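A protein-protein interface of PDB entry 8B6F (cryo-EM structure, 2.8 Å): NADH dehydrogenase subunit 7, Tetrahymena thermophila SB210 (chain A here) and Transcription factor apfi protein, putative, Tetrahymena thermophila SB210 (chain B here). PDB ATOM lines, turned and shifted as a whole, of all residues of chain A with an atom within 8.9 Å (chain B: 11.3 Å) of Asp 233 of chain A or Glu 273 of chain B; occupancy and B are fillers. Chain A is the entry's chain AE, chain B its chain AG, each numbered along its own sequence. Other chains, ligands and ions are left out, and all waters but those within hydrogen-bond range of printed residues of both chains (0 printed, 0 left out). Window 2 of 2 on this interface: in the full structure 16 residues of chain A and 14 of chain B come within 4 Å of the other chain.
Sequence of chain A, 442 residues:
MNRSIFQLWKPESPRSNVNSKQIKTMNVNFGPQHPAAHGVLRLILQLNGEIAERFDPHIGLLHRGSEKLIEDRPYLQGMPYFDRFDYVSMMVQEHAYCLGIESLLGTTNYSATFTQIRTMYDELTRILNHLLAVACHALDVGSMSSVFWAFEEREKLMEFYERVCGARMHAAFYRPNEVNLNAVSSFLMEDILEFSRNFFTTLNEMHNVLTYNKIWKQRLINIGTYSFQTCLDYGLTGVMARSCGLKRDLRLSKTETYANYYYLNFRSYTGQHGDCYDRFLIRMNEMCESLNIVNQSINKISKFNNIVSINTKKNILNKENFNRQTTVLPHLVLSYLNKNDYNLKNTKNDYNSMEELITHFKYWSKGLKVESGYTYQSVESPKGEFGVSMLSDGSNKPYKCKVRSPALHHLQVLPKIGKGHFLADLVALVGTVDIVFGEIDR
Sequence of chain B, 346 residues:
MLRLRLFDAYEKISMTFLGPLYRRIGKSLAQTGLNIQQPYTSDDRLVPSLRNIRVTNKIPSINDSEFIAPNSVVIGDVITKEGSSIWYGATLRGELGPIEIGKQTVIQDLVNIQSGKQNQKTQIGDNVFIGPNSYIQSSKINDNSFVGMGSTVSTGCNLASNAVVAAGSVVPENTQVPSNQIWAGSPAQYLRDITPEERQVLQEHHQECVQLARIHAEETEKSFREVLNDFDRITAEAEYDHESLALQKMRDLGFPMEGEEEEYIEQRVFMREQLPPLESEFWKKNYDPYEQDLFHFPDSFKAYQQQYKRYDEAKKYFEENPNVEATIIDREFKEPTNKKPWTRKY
Hydrophobic or aromatic side chains of chain B within 4 Å of the printed part of chain A: Phe 270 and Met 271.
Printed residues of chain A that touch a printed residue of chain B: Thr 230, Asp 233, Tyr 234 and Lys 416.
Hydrophobic or aromatic side chains of chain A within 4 Å of the printed part of chain B: Tyr 234.
Among the printed residues, 6 pairs touch across the chains.
NZ of Lys 416 of chain A lies within hydrogen-bond range of O of Phe 270 of chain B (2.8 Å).
The side-chain amino group (NZ) of Lys 416 of chain A sits at hydrogen-bond distance from the backbone carbonyl oxygen (O) of Met 271 of chain B (3.2 Å).
NZ of Lys 416 of chain A is in salt-bridge range of OE2 of Glu 273 of chain B.
Asp 233 of chain A touches just one residue of chain B: Glu 273 (3.1 Å).
Glu 273 of chain B touches three residues of chain A.
Thr 230 of chain A touches just one residue of chain B: Met 271.
No residue of chain B comes within 4 Å of Leu 232 of chain A.
Of chain B, only Glu 273 comes within 4 Å of Tyr 234 of chain A.
Printed residues of chain A within 4 Å of Phe 270 of chain B: Lys 416 (2.8 Å).
Printed residues of chain A within 4 Å of Met 271 of chain B: Thr 230 (3.97 Å) and Lys 416 (3.2 Å).
Of the printed residues of chain B, Lys 416 of chain A touches Phe 270, Met 271 and Glu 273.
His 409 of chain A touches none of the printed residues of chain B.
Val 269 of chain B touches none of the printed residues of chain A.
Among the printed residues, merely in contact across the chains: Thr 230 of chain A with Met 271 of chain B, Asp 233 of chain A with Glu 273 of chain B and Tyr 234 of chain A with Glu 273 of chain B.
OD1 of Asp 233 of chain A lies within hydrogen-bond range of NE2 of Gln 229 of chain A, at 2.6 Å.
The backbone carbonyl oxygen of Glu 266 of chain B is in hydrogen-bond range of the backbone NH of Met 271 of chain B, 2.8 Å away.
The side-chain sulfur of Cys 244 of chain A forms a disulfide with the side-chain sulfur of Cys 231 of chain A (2.1 Å).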
ATOM      1  N   SER A 227      -3.970   5.687 -21.012  1.00  0.00           N
ATOM      2  CA  SER A 227      -4.650   4.418 -20.804  1.00  0.00           C
ATOM      3  C   SER A 227      -6.050   4.593 -20.219  1.00  0.00           C
ATOM      4  O   SER A 227      -6.479   5.688 -19.853  1.00  0.00           O
ATOM      5  CB  SER A 227      -3.826   3.520 -19.884  1.00  0.00           C
ATOM      6  OG  SER A 227      -4.239   2.170 -19.996  1.00  0.00           O
ATOM      7  N   PHE A 228      -6.759   3.465 -20.134  1.00  0.00           N
ATOM      8  CA  PHE A 228      -8.091   3.441 -19.539  1.00  0.00           C
ATOM      9  C   PHE A 228      -8.004   3.885 -18.083  1.00  0.00           C
ATOM     10  O   PHE A 228      -8.898   4.570 -17.575  1.00  0.00           O
ATOM     11  CB  PHE A 228      -8.727   2.054 -19.690  1.00  0.00           C
ATOM     12  CG  PHE A 228      -8.112   0.991 -18.831  1.00  0.00           C
ATOM     13  CD1 PHE A 228      -7.033   0.250 -19.283  1.00  0.00           C
ATOM     14  CD2 PHE A 228      -8.656   0.689 -17.595  1.00  0.00           C
ATOM     15  CE1 PHE A 228      -6.481  -0.743 -18.498  1.00  0.00           C
ATOM     16  CE2 PHE A 228      -8.108  -0.300 -16.806  1.00  0.00           C
ATOM     17  CZ  PHE A 228      -7.021  -1.018 -17.258  1.00  0.00           C
ATOM     18  N   GLN A 229      -6.933   3.486 -17.395  1.00  0.00           N
ATOM     19  CA  GLN A 229      -6.776   3.774 -15.972  1.00  0.00           C
ATOM     20  C   GLN A 229      -6.722   5.283 -15.750  1.00  0.00           C
ATOM     21  O   GLN A 229      -7.330   5.800 -14.809  1.00  0.00           O
ATOM     22  CB  GLN A 229      -5.537   3.085 -15.410  1.00  0.00           C
ATOM     23  CG  GLN A 229      -5.461   3.155 -13.889  1.00  0.00           C
ATOM     24  CD  GLN A 229      -6.645   2.483 -13.216  1.00  0.00           C
ATOM     25  OE1 GLN A 229      -7.296   1.620 -13.800  1.00  0.00           O
ATOM     26  NE2 GLN A 229      -6.938   2.888 -11.987  1.00  0.00           N
ATOM     27  N   THR A 230      -6.011   6.011 -16.618  1.00  0.00           N
ATOM     28  CA  THR A 230      -6.037   7.469 -16.535  1.00  0.00           C
ATOM     29  C   THR A 230      -7.454   7.930 -16.822  1.00  0.00           C
ATOM     30  O   THR A 230      -7.963   8.853 -16.175  1.00  0.00           O
ATOM     31  CB  THR A 230      -5.052   8.092 -17.522  1.00  0.00           C
ATOM     32  OG1 THR A 230      -3.720   7.676 -17.203  1.00  0.00           O
ATOM     33  CG2 THR A 230      -5.135   9.613 -17.484  1.00  0.00           C
ATOM     34  N   CYS A 231      -8.103   7.298 -17.793  1.00  0.00           N
ATOM     35  CA  CYS A 231      -9.442   7.697 -18.192  1.00  0.00           C
ATOM     36  C   CYS A 231     -10.358   7.526 -16.976  1.00  0.00           C
ATOM     37  O   CYS A 231     -11.186   8.389 -16.669  1.00  0.00           O
ATOM     38  CB  CYS A 231      -9.926   6.856 -19.394  1.00  0.00           C
ATOM     39  SG  CYS A 231      -9.772   7.539 -21.133  1.00  0.00           S
ATOM     40  N   LEU A 232     -10.198   6.396 -16.279  1.00  0.00           N
ATOM     41  CA  LEU A 232     -10.908   6.052 -15.043  1.00  0.00           C
ATOM     42  C   LEU A 232     -10.513   6.907 -13.829  1.00  0.00           C
ATOM     43  O   LEU A 232     -11.384   7.372 -13.084  1.00  0.00           O
ATOM     44  CB  LEU A 232     -10.612   4.590 -14.712  1.00  0.00           C
ATOM     45  CG  LEU A 232     -11.556   3.794 -13.820  1.00  0.00           C
ATOM     46  CD1 LEU A 232     -12.796   3.351 -14.565  1.00  0.00           C
ATOM     47  CD2 LEU A 232     -10.805   2.615 -13.239  1.00  0.00           C
ATOM     48  N   ASP A 233      -9.215   7.135 -13.610  1.00  0.00           N
ATOM     49  CA  ASP A 233      -8.747   7.858 -12.419  1.00  0.00           C
ATOM     50  C   ASP A 233      -9.180   9.320 -12.396  1.00  0.00           C
ATOM     51  O   ASP A 233      -9.553   9.840 -11.338  1.00  0.00           O
ATOM     52  CB  ASP A 233      -7.224   7.780 -12.306  1.00  0.00           C
ATOM     53  CG  ASP A 233      -6.726   6.369 -12.095  1.00  0.00           C
ATOM     54  OD1 ASP A 233      -7.508   5.420 -12.308  1.00  0.00           O
ATOM     55  OD2 ASP A 233      -5.550   6.206 -11.706  1.00  0.00           O
ATOM     56  N   TYR A 234      -9.142   9.996 -13.530  1.00  0.00           N
ATOM     57  CA  TYR A 234      -9.418  11.422 -13.637  1.00  0.00           C
ATOM     58  C   TYR A 234     -10.841  11.710 -14.100  1.00  0.00           C
ATOM     59  O   TYR A 234     -11.165  12.859 -14.412  1.00  0.00           O
ATOM     60  CB  TYR A 234      -8.394  12.090 -14.544  1.00  0.00           C
ATOM     61  CG  TYR A 234      -7.109  12.410 -13.814  1.00  0.00           C
ATOM     62  CD1 TYR A 234      -6.121  11.452 -13.648  1.00  0.00           C
ATOM     63  CD2 TYR A 234      -6.896  13.672 -13.272  1.00  0.00           C
ATOM     64  CE1 TYR A 234      -4.952  11.742 -12.973  1.00  0.00           C
ATOM     65  CE2 TYR A 234      -5.731  13.973 -12.597  1.00  0.00           C
ATOM     66  CZ  TYR A 234      -4.761  13.006 -12.457  1.00  0.00           C
ATOM     67  OH  TYR A 234      -3.601  13.298 -11.779  1.00  0.00           O
ATOM     68  N   GLY A 235     -11.687  10.687 -14.150  1.00  0.00           N
ATOM     69  CA  GLY A 235     -13.073  10.824 -14.571  1.00  0.00           C
ATOM     70  C   GLY A 235     -13.268  11.347 -15.973  1.00  0.00           C
ATOM     71  O   GLY A 235     -14.208  12.106 -16.240  1.00  0.00           O
ATOM     72  N   LEU A 236     -12.379  10.951 -16.874  1.00  0.00           N
ATOM     73  CA  LEU A 236     -12.445  11.337 -18.273  1.00  0.00           C
ATOM     74  C   LEU A 236     -13.689  10.691 -18.869  1.00  0.00           C
ATOM     75  O   LEU A 236     -14.066   9.579 -18.493  1.00  0.00           O
ATOM     76  CB  LEU A 236     -11.170  10.929 -19.000  1.00  0.00           C
ATOM     77  CG  LEU A 236      -9.906  11.534 -18.374  1.00  0.00           C
ATOM     78  CD1 LEU A 236      -8.699  11.339 -19.271  1.00  0.00           C
ATOM     79  CD2 LEU A 236     -10.091  13.020 -18.046  1.00  0.00           C
ATOM     80  N   CYS A 244      -9.781   6.002 -25.282  1.00  0.00           N
ATOM     81  CA  CYS A 244      -9.111   4.894 -24.605  1.00  0.00           C
ATOM     82  C   CYS A 244      -9.764   3.552 -24.909  1.00  0.00           C
ATOM     83  O   CYS A 244      -9.250   2.519 -24.472  1.00  0.00           O
ATOM     84  CB  CYS A 244      -9.123   5.059 -23.060  1.00  0.00           C
ATOM     85  SG  CYS A 244      -8.367   6.518 -22.229  1.00  0.00           S
ATOM     86  N   LEU A 246     -12.837   2.777 -23.857  1.00  0.00           N
ATOM     87  CA  LEU A 246     -13.742   2.418 -22.771  1.00  0.00           C
ATOM     88  C   LEU A 246     -15.122   2.036 -23.281  1.00  0.00           C
ATOM     89  O   LEU A 246     -15.840   1.282 -22.613  1.00  0.00           O
ATOM     90  CB  LEU A 246     -13.850   3.572 -21.779  1.00  0.00           C
ATOM     91  CG  LEU A 246     -12.693   3.706 -20.787  1.00  0.00           C
ATOM     92  CD1 LEU A 246     -12.828   4.995 -20.018  1.00  0.00           C
ATOM     93  CD2 LEU A 246     -12.624   2.530 -19.829  1.00  0.00           C
ATOM     94  N   HIS A 409     -13.089  18.238 -15.437  1.00  0.00           N
ATOM     95  CA  HIS A 409     -12.335  16.992 -15.338  1.00  0.00           C
ATOM     96  C   HIS A 409     -11.337  16.856 -16.481  1.00  0.00           C
ATOM     97  O   HIS A 409     -10.231  16.340 -16.287  1.00  0.00           O
ATOM     98  CB  HIS A 409     -13.292  15.801 -15.309  1.00  0.00           C
ATOM     99  CG  HIS A 409     -14.154  15.752 -14.087  1.00  0.00           C
ATOM    100  ND1 HIS A 409     -15.095  16.717 -13.798  1.00  0.00           N
ATOM    101  CD2 HIS A 409     -14.216  14.853 -13.077  1.00  0.00           C
ATOM    102  CE1 HIS A 409     -15.699  16.413 -12.664  1.00  0.00           C
ATOM    103  NE2 HIS A 409     -15.185  15.287 -12.205  1.00  0.00           N
ATOM    104  N   GLN A 412      -8.415  18.928 -15.650  1.00  0.00           N
ATOM    105  CA  GLN A 412      -7.629  18.394 -14.543  1.00  0.00           C
ATOM    106  C   GLN A 412      -6.473  17.536 -15.041  1.00  0.00           C
ATOM    107  O   GLN A 412      -5.389  17.542 -14.448  1.00  0.00           O
ATOM    108  CB  GLN A 412      -8.521  17.579 -13.608  1.00  0.00           C
ATOM    109  CG  GLN A 412      -9.244  18.397 -12.563  1.00  0.00           C
ATOM    110  CD  GLN A 412      -9.208  17.742 -11.199  1.00  0.00           C
ATOM    111  OE1 GLN A 412      -8.137  17.457 -10.665  1.00  0.00           O
ATOM    112  NE2 GLN A 412     -10.380  17.492 -10.633  1.00  0.00           N
ATOM    113  N   VAL A 413      -6.692  16.765 -16.110  1.00  0.00           N
ATOM    114  CA  VAL A 413      -5.649  15.868 -16.610  1.00  0.00           C
ATOM    115  C   VAL A 413      -4.591  16.575 -17.432  1.00  0.00           C
ATOM    116  O   VAL A 413      -3.565  15.963 -17.750  1.00  0.00           O
ATOM    117  CB  VAL A 413      -6.186  14.730 -17.498  1.00  0.00           C
ATOM    118  CG1 VAL A 413      -6.864  13.710 -16.660  1.00  0.00           C
ATOM    119  CG2 VAL A 413      -7.146  15.261 -18.551  1.00  0.00           C
ATOM    120  N   LYS A 416      -1.169  16.074 -16.334  1.00  0.00           N
ATOM    121  CA  LYS A 416      -0.752  14.678 -16.436  1.00  0.00           C
ATOM    122  C   LYS A 416      -0.354  14.319 -17.861  1.00  0.00           C
ATOM    123  O   LYS A 416       0.702  13.721 -18.093  1.00  0.00           O
ATOM    124  CB  LYS A 416      -1.872  13.758 -15.953  1.00  0.00           C
ATOM    125  CG  LYS A 416      -1.990  13.658 -14.446  1.00  0.00           C
ATOM    126  CD  LYS A 416      -0.844  12.872 -13.821  1.00  0.00           C
ATOM    127  CE  LYS A 416      -0.900  11.399 -14.189  1.00  0.00           C
ATOM    128  NZ  LYS A 416       0.109  10.606 -13.435  1.00  0.00           N
ATOM    129  N   LEU B 253      12.106  -1.728 -11.985  1.00  0.00           N
ATOM    130  CA  LEU B 253      10.915  -0.902 -11.822  1.00  0.00           C
ATOM    131  C   LEU B 253       9.986  -1.008 -13.024  1.00  0.00           C
ATOM    132  O   LEU B 253       8.773  -0.815 -12.884  1.00  0.00           O
ATOM    133  CB  LEU B 253      11.313   0.556 -11.591  1.00  0.00           C
ATOM    134  CG  LEU B 253      11.491   0.981 -10.131  1.00  0.00           C
ATOM    135  CD1 LEU B 253      12.510   0.119  -9.401  1.00  0.00           C
ATOM    136  CD2 LEU B 253      11.895   2.443 -10.069  1.00  0.00           C
ATOM    137  N   ILE B 265       7.627   6.094 -22.418  1.00  0.00           N
ATOM    138  CA  ILE B 265       8.247   6.275 -21.109  1.00  0.00           C
ATOM    139  C   ILE B 265       7.242   6.831 -20.109  1.00  0.00           C
ATOM    140  O   ILE B 265       7.185   6.389 -18.955  1.00  0.00           O
ATOM    141  CB  ILE B 265       9.492   7.175 -21.230  1.00  0.00           C
ATOM    142  CG1 ILE B 265      10.191   7.296 -19.872  1.00  0.00           C
ATOM    143  CG2 ILE B 265       9.117   8.554 -21.781  1.00  0.00           C
ATOM    144  CD1 ILE B 265      11.481   8.094 -19.903  1.00  0.00           C
ATOM    145  N   GLU B 266       6.435   7.809 -20.527  1.00  0.00           N
ATOM    146  CA  GLU B 266       5.528   8.462 -19.589  1.00  0.00           C
ATOM    147  C   GLU B 266       4.547   7.477 -18.970  1.00  0.00           C
ATOM    148  O   GLU B 266       4.099   7.678 -17.836  1.00  0.00           O
ATOM    149  CB  GLU B 266       4.771   9.601 -20.280  1.00  0.00           C
ATOM    150  CG  GLU B 266       3.790   9.176 -21.371  1.00  0.00           C
ATOM    151  CD  GLU B 266       4.469   8.822 -22.676  1.00  0.00           C
ATOM    152  OE1 GLU B 266       5.712   8.913 -22.743  1.00  0.00           O
ATOM    153  OE2 GLU B 266       3.761   8.458 -23.639  1.00  0.00           O
ATOM    154  N   GLN B 267       4.203   6.408 -19.690  1.00  0.00           N
ATOM    155  CA  GLN B 267       3.280   5.415 -19.155  1.00  0.00           C
ATOM    156  C   GLN B 267       3.884   4.591 -18.030  1.00  0.00           C
ATOM    157  O   GLN B 267       3.143   3.917 -17.310  1.00  0.00           O
ATOM    158  CB  GLN B 267       2.812   4.480 -20.267  1.00  0.00           C
ATOM    159  CG  GLN B 267       1.524   4.906 -20.925  1.00  0.00           C
ATOM    160  CD  GLN B 267       1.646   6.210 -21.677  1.00  0.00           C
ATOM    161  OE1 GLN B 267       2.630   6.447 -22.373  1.00  0.00           O
ATOM    162  NE2 GLN B 267       0.643   7.066 -21.537  1.00  0.00           N
ATOM    163  N   ARG B 268       5.206   4.622 -17.863  1.00  0.00           N
ATOM    164  CA  ARG B 268       5.875   3.805 -16.864  1.00  0.00           C
ATOM    165  C   ARG B 268       6.557   4.601 -15.764  1.00  0.00           C
ATOM    166  O   ARG B 268       6.898   4.015 -14.731  1.00  0.00           O
ATOM    167  CB  ARG B 268       6.928   2.904 -17.531  1.00  0.00           C
ATOM    168  CG  ARG B 268       6.381   1.580 -18.036  1.00  0.00           C
ATOM    169  CD  ARG B 268       5.990   0.667 -16.885  1.00  0.00           C
ATOM    170  NE  ARG B 268       5.872  -0.723 -17.307  1.00  0.00           N
ATOM    171  CZ  ARG B 268       4.761  -1.282 -17.767  1.00  0.00           C
ATOM    172  NH1 ARG B 268       3.636  -0.595 -17.881  1.00  0.00           N
ATOM    173  NH2 ARG B 268       4.780  -2.562 -18.124  1.00  0.00           N
ATOM    174  N   VAL B 269       6.758   5.903 -15.945  1.00  0.00           N
ATOM    175  CA  VAL B 269       7.467   6.725 -14.979  1.00  0.00           C
ATOM    176  C   VAL B 269       6.533   7.708 -14.285  1.00  0.00           C
ATOM    177  O   VAL B 269       6.667   7.948 -13.082  1.00  0.00           O
ATOM    178  CB  VAL B 269       8.649   7.464 -15.649  1.00  0.00           C
ATOM    179  CG1 VAL B 269       9.558   6.477 -16.362  1.00  0.00           C
ATOM    180  CG2 VAL B 269       8.157   8.531 -16.618  1.00  0.00           C
ATOM    181  N   PHE B 270       5.582   8.279 -15.016  1.00  0.00           N
ATOM    182  CA  PHE B 270       4.745   9.357 -14.503  1.00  0.00           C
ATOM    183  C   PHE B 270       3.268   9.010 -14.444  1.00  0.00           C
ATOM    184  O   PHE B 270       2.590   9.397 -13.489  1.00  0.00           O
ATOM    185  CB  PHE B 270       4.940  10.612 -15.368  1.00  0.00           C
ATOM    186  CG  PHE B 270       4.140  11.794 -14.909  1.00  0.00           C
ATOM    187  CD1 PHE B 270       4.228  12.240 -13.600  1.00  0.00           C
ATOM    188  CD2 PHE B 270       3.318  12.473 -15.789  1.00  0.00           C
ATOM    189  CE1 PHE B 270       3.499  13.330 -13.176  1.00  0.00           C
ATOM    190  CE2 PHE B 270       2.586  13.564 -15.371  1.00  0.00           C
ATOM    191  CZ  PHE B 270       2.676  13.993 -14.063  1.00  0.00           C
ATOM    192  N   MET B 271       2.745   8.289 -15.437  1.00  0.00           N
ATOM    193  CA  MET B 271       1.308   8.035 -15.482  1.00  0.00           C
ATOM    194  C   MET B 271       0.845   7.208 -14.289  1.00  0.00           C
ATOM    195  O   MET B 271      -0.222   7.473 -13.723  1.00  0.00           O
ATOM    196  CB  MET B 271       0.943   7.335 -16.790  1.00  0.00           C
ATOM    197  CG  MET B 271       0.961   8.254 -18.004  1.00  0.00           C
ATOM    198  SD  MET B 271      -0.293   9.544 -17.922  1.00  0.00           S
ATOM    199  CE  MET B 271       0.014  10.414 -19.454  1.00  0.00           C
ATOM    200  N   ARG B 272       1.621   6.199 -13.896  1.00  0.00           N
ATOM    201  CA  ARG B 272       1.210   5.337 -12.795  1.00  0.00           C
ATOM    202  C   ARG B 272       0.998   6.155 -11.529  1.00  0.00           C
ATOM    203  O   ARG B 272       1.863   6.937 -11.124  1.00  0.00           O
ATOM    204  CB  ARG B 272       2.253   4.247 -12.553  1.00  0.00           C
ATOM    205  CG  ARG B 272       2.194   3.115 -13.563  1.00  0.00           C
ATOM    206  CD  ARG B 272       3.110   1.966 -13.178  1.00  0.00           C
ATOM    207  NE  ARG B 272       4.515   2.289 -13.393  1.00  0.00           N
ATOM    208  CZ  ARG B 272       5.518   1.449 -13.176  1.00  0.00           C
ATOM    209  NH1 ARG B 272       5.310   0.224 -12.721  1.00  0.00           N
ATOM    210  NH2 ARG B 272       6.763   1.848 -13.423  1.00  0.00           N
ATOM    211  N   GLU B 273      -0.158   5.969 -10.899  1.00  0.00           N
ATOM    212  CA  GLU B 273      -0.492   6.713  -9.697  1.00  0.00           C
ATOM    213  C   GLU B 273       0.273   6.167  -8.497  1.00  0.00           C
ATOM    214  O   GLU B 273       0.719   5.018  -8.475  1.00  0.00           O
ATOM    215  CB  GLU B 273      -1.994   6.647  -9.425  1.00  0.00           C
ATOM    216  CG  GLU B 273      -2.845   7.250 -10.524  1.00  0.00           C
ATOM    217  CD  GLU B 273      -2.585   8.731 -10.713  1.00  0.00           C
ATOM    218  OE1 GLU B 273      -2.162   9.390  -9.742  1.00  0.00           O
ATOM    219  OE2 GLU B 273      -2.800   9.233 -11.835  1.00  0.00           O
ATOM    220  N   GLN B 274       0.421   7.018  -7.487  1.00  0.00           N
ATOM    221  CA  GLN B 274       1.110   6.649  -6.261  1.00  0.00           C
ATOM    222  C   GLN B 274       0.128   6.055  -5.265  1.00  0.00           C
ATOM    223  O   GLN B 274      -1.016   6.503  -5.156  1.00  0.00           O
ATOM    224  CB  GLN B 274       1.806   7.865  -5.653  1.00  0.00           C
ATOM    225  CG  GLN B 274       2.890   8.429  -6.547  1.00  0.00           C
ATOM    226  CD  GLN B 274       3.716   9.489  -5.861  1.00  0.00           C
ATOM    227  OE1 GLN B 274       3.359   9.980  -4.792  1.00  0.00           O
ATOM    228  NE2 GLN B 274       4.837   9.847  -6.475  1.00  0.00           N
ATOM    229  N   LEU B 275       0.583   5.044  -4.540  1.00  0.00           N
ATOM    230  CA  LEU B 275      -0.284   4.367  -3.590  1.00  0.00           C
ATOM    231  C   LEU B 275      -0.726   5.344  -2.504  1.00  0.00           C
ATOM    232  O   LEU B 275       0.119   6.032  -1.917  1.00  0.00           O
ATOM    233  CB  LEU B 275       0.448   3.175  -2.975  1.00  0.00           C
ATOM    234  CG  LEU B 275       0.819   2.042  -3.933  1.00  0.00           C
ATOM    235  CD1 LEU B 275       1.721   1.036  -3.243  1.00  0.00           C
ATOM    236  CD2 LEU B 275      -0.429   1.356  -4.463  1.00  0.00           C
ATOM    237  N   PRO B 276      -2.026   5.436  -2.204  1.00  0.00           N
ATOM    238  CA  PRO B 276      -2.466   6.393  -1.193  1.00  0.00           C
ATOM    239  C   PRO B 276      -1.923   6.023   0.175  1.00  0.00           C
ATOM    240  O   PRO B 276      -1.646   4.844   0.451  1.00  0.00           O
ATOM    241  CB  PRO B 276      -4.000   6.279  -1.241  1.00  0.00           C
ATOM    242  CG  PRO B 276      -4.263   4.939  -1.792  1.00  0.00           C
ATOM    243  CD  PRO B 276      -3.155   4.673  -2.763  1.00  0.00           C
ATOM    244  N   PRO B 277      -1.747   6.999   1.065  1.00  0.00           N
ATOM    245  CA  PRO B 277      -1.199   6.688   2.389  1.00  0.00           C
ATOM    246  C   PRO B 277      -2.089   5.724   3.158  1.00  0.00           C
ATOM    247  O   PRO B 277      -3.315   5.740   3.036  1.00  0.00           O
ATOM    248  CB  PRO B 277      -1.137   8.055   3.082  1.00  0.00           C
ATOM    249  CG  PRO B 277      -1.191   9.055   1.988  1.00  0.00           C
ATOM    250  CD  PRO B 277      -2.015   8.438   0.907  1.00  0.00           C
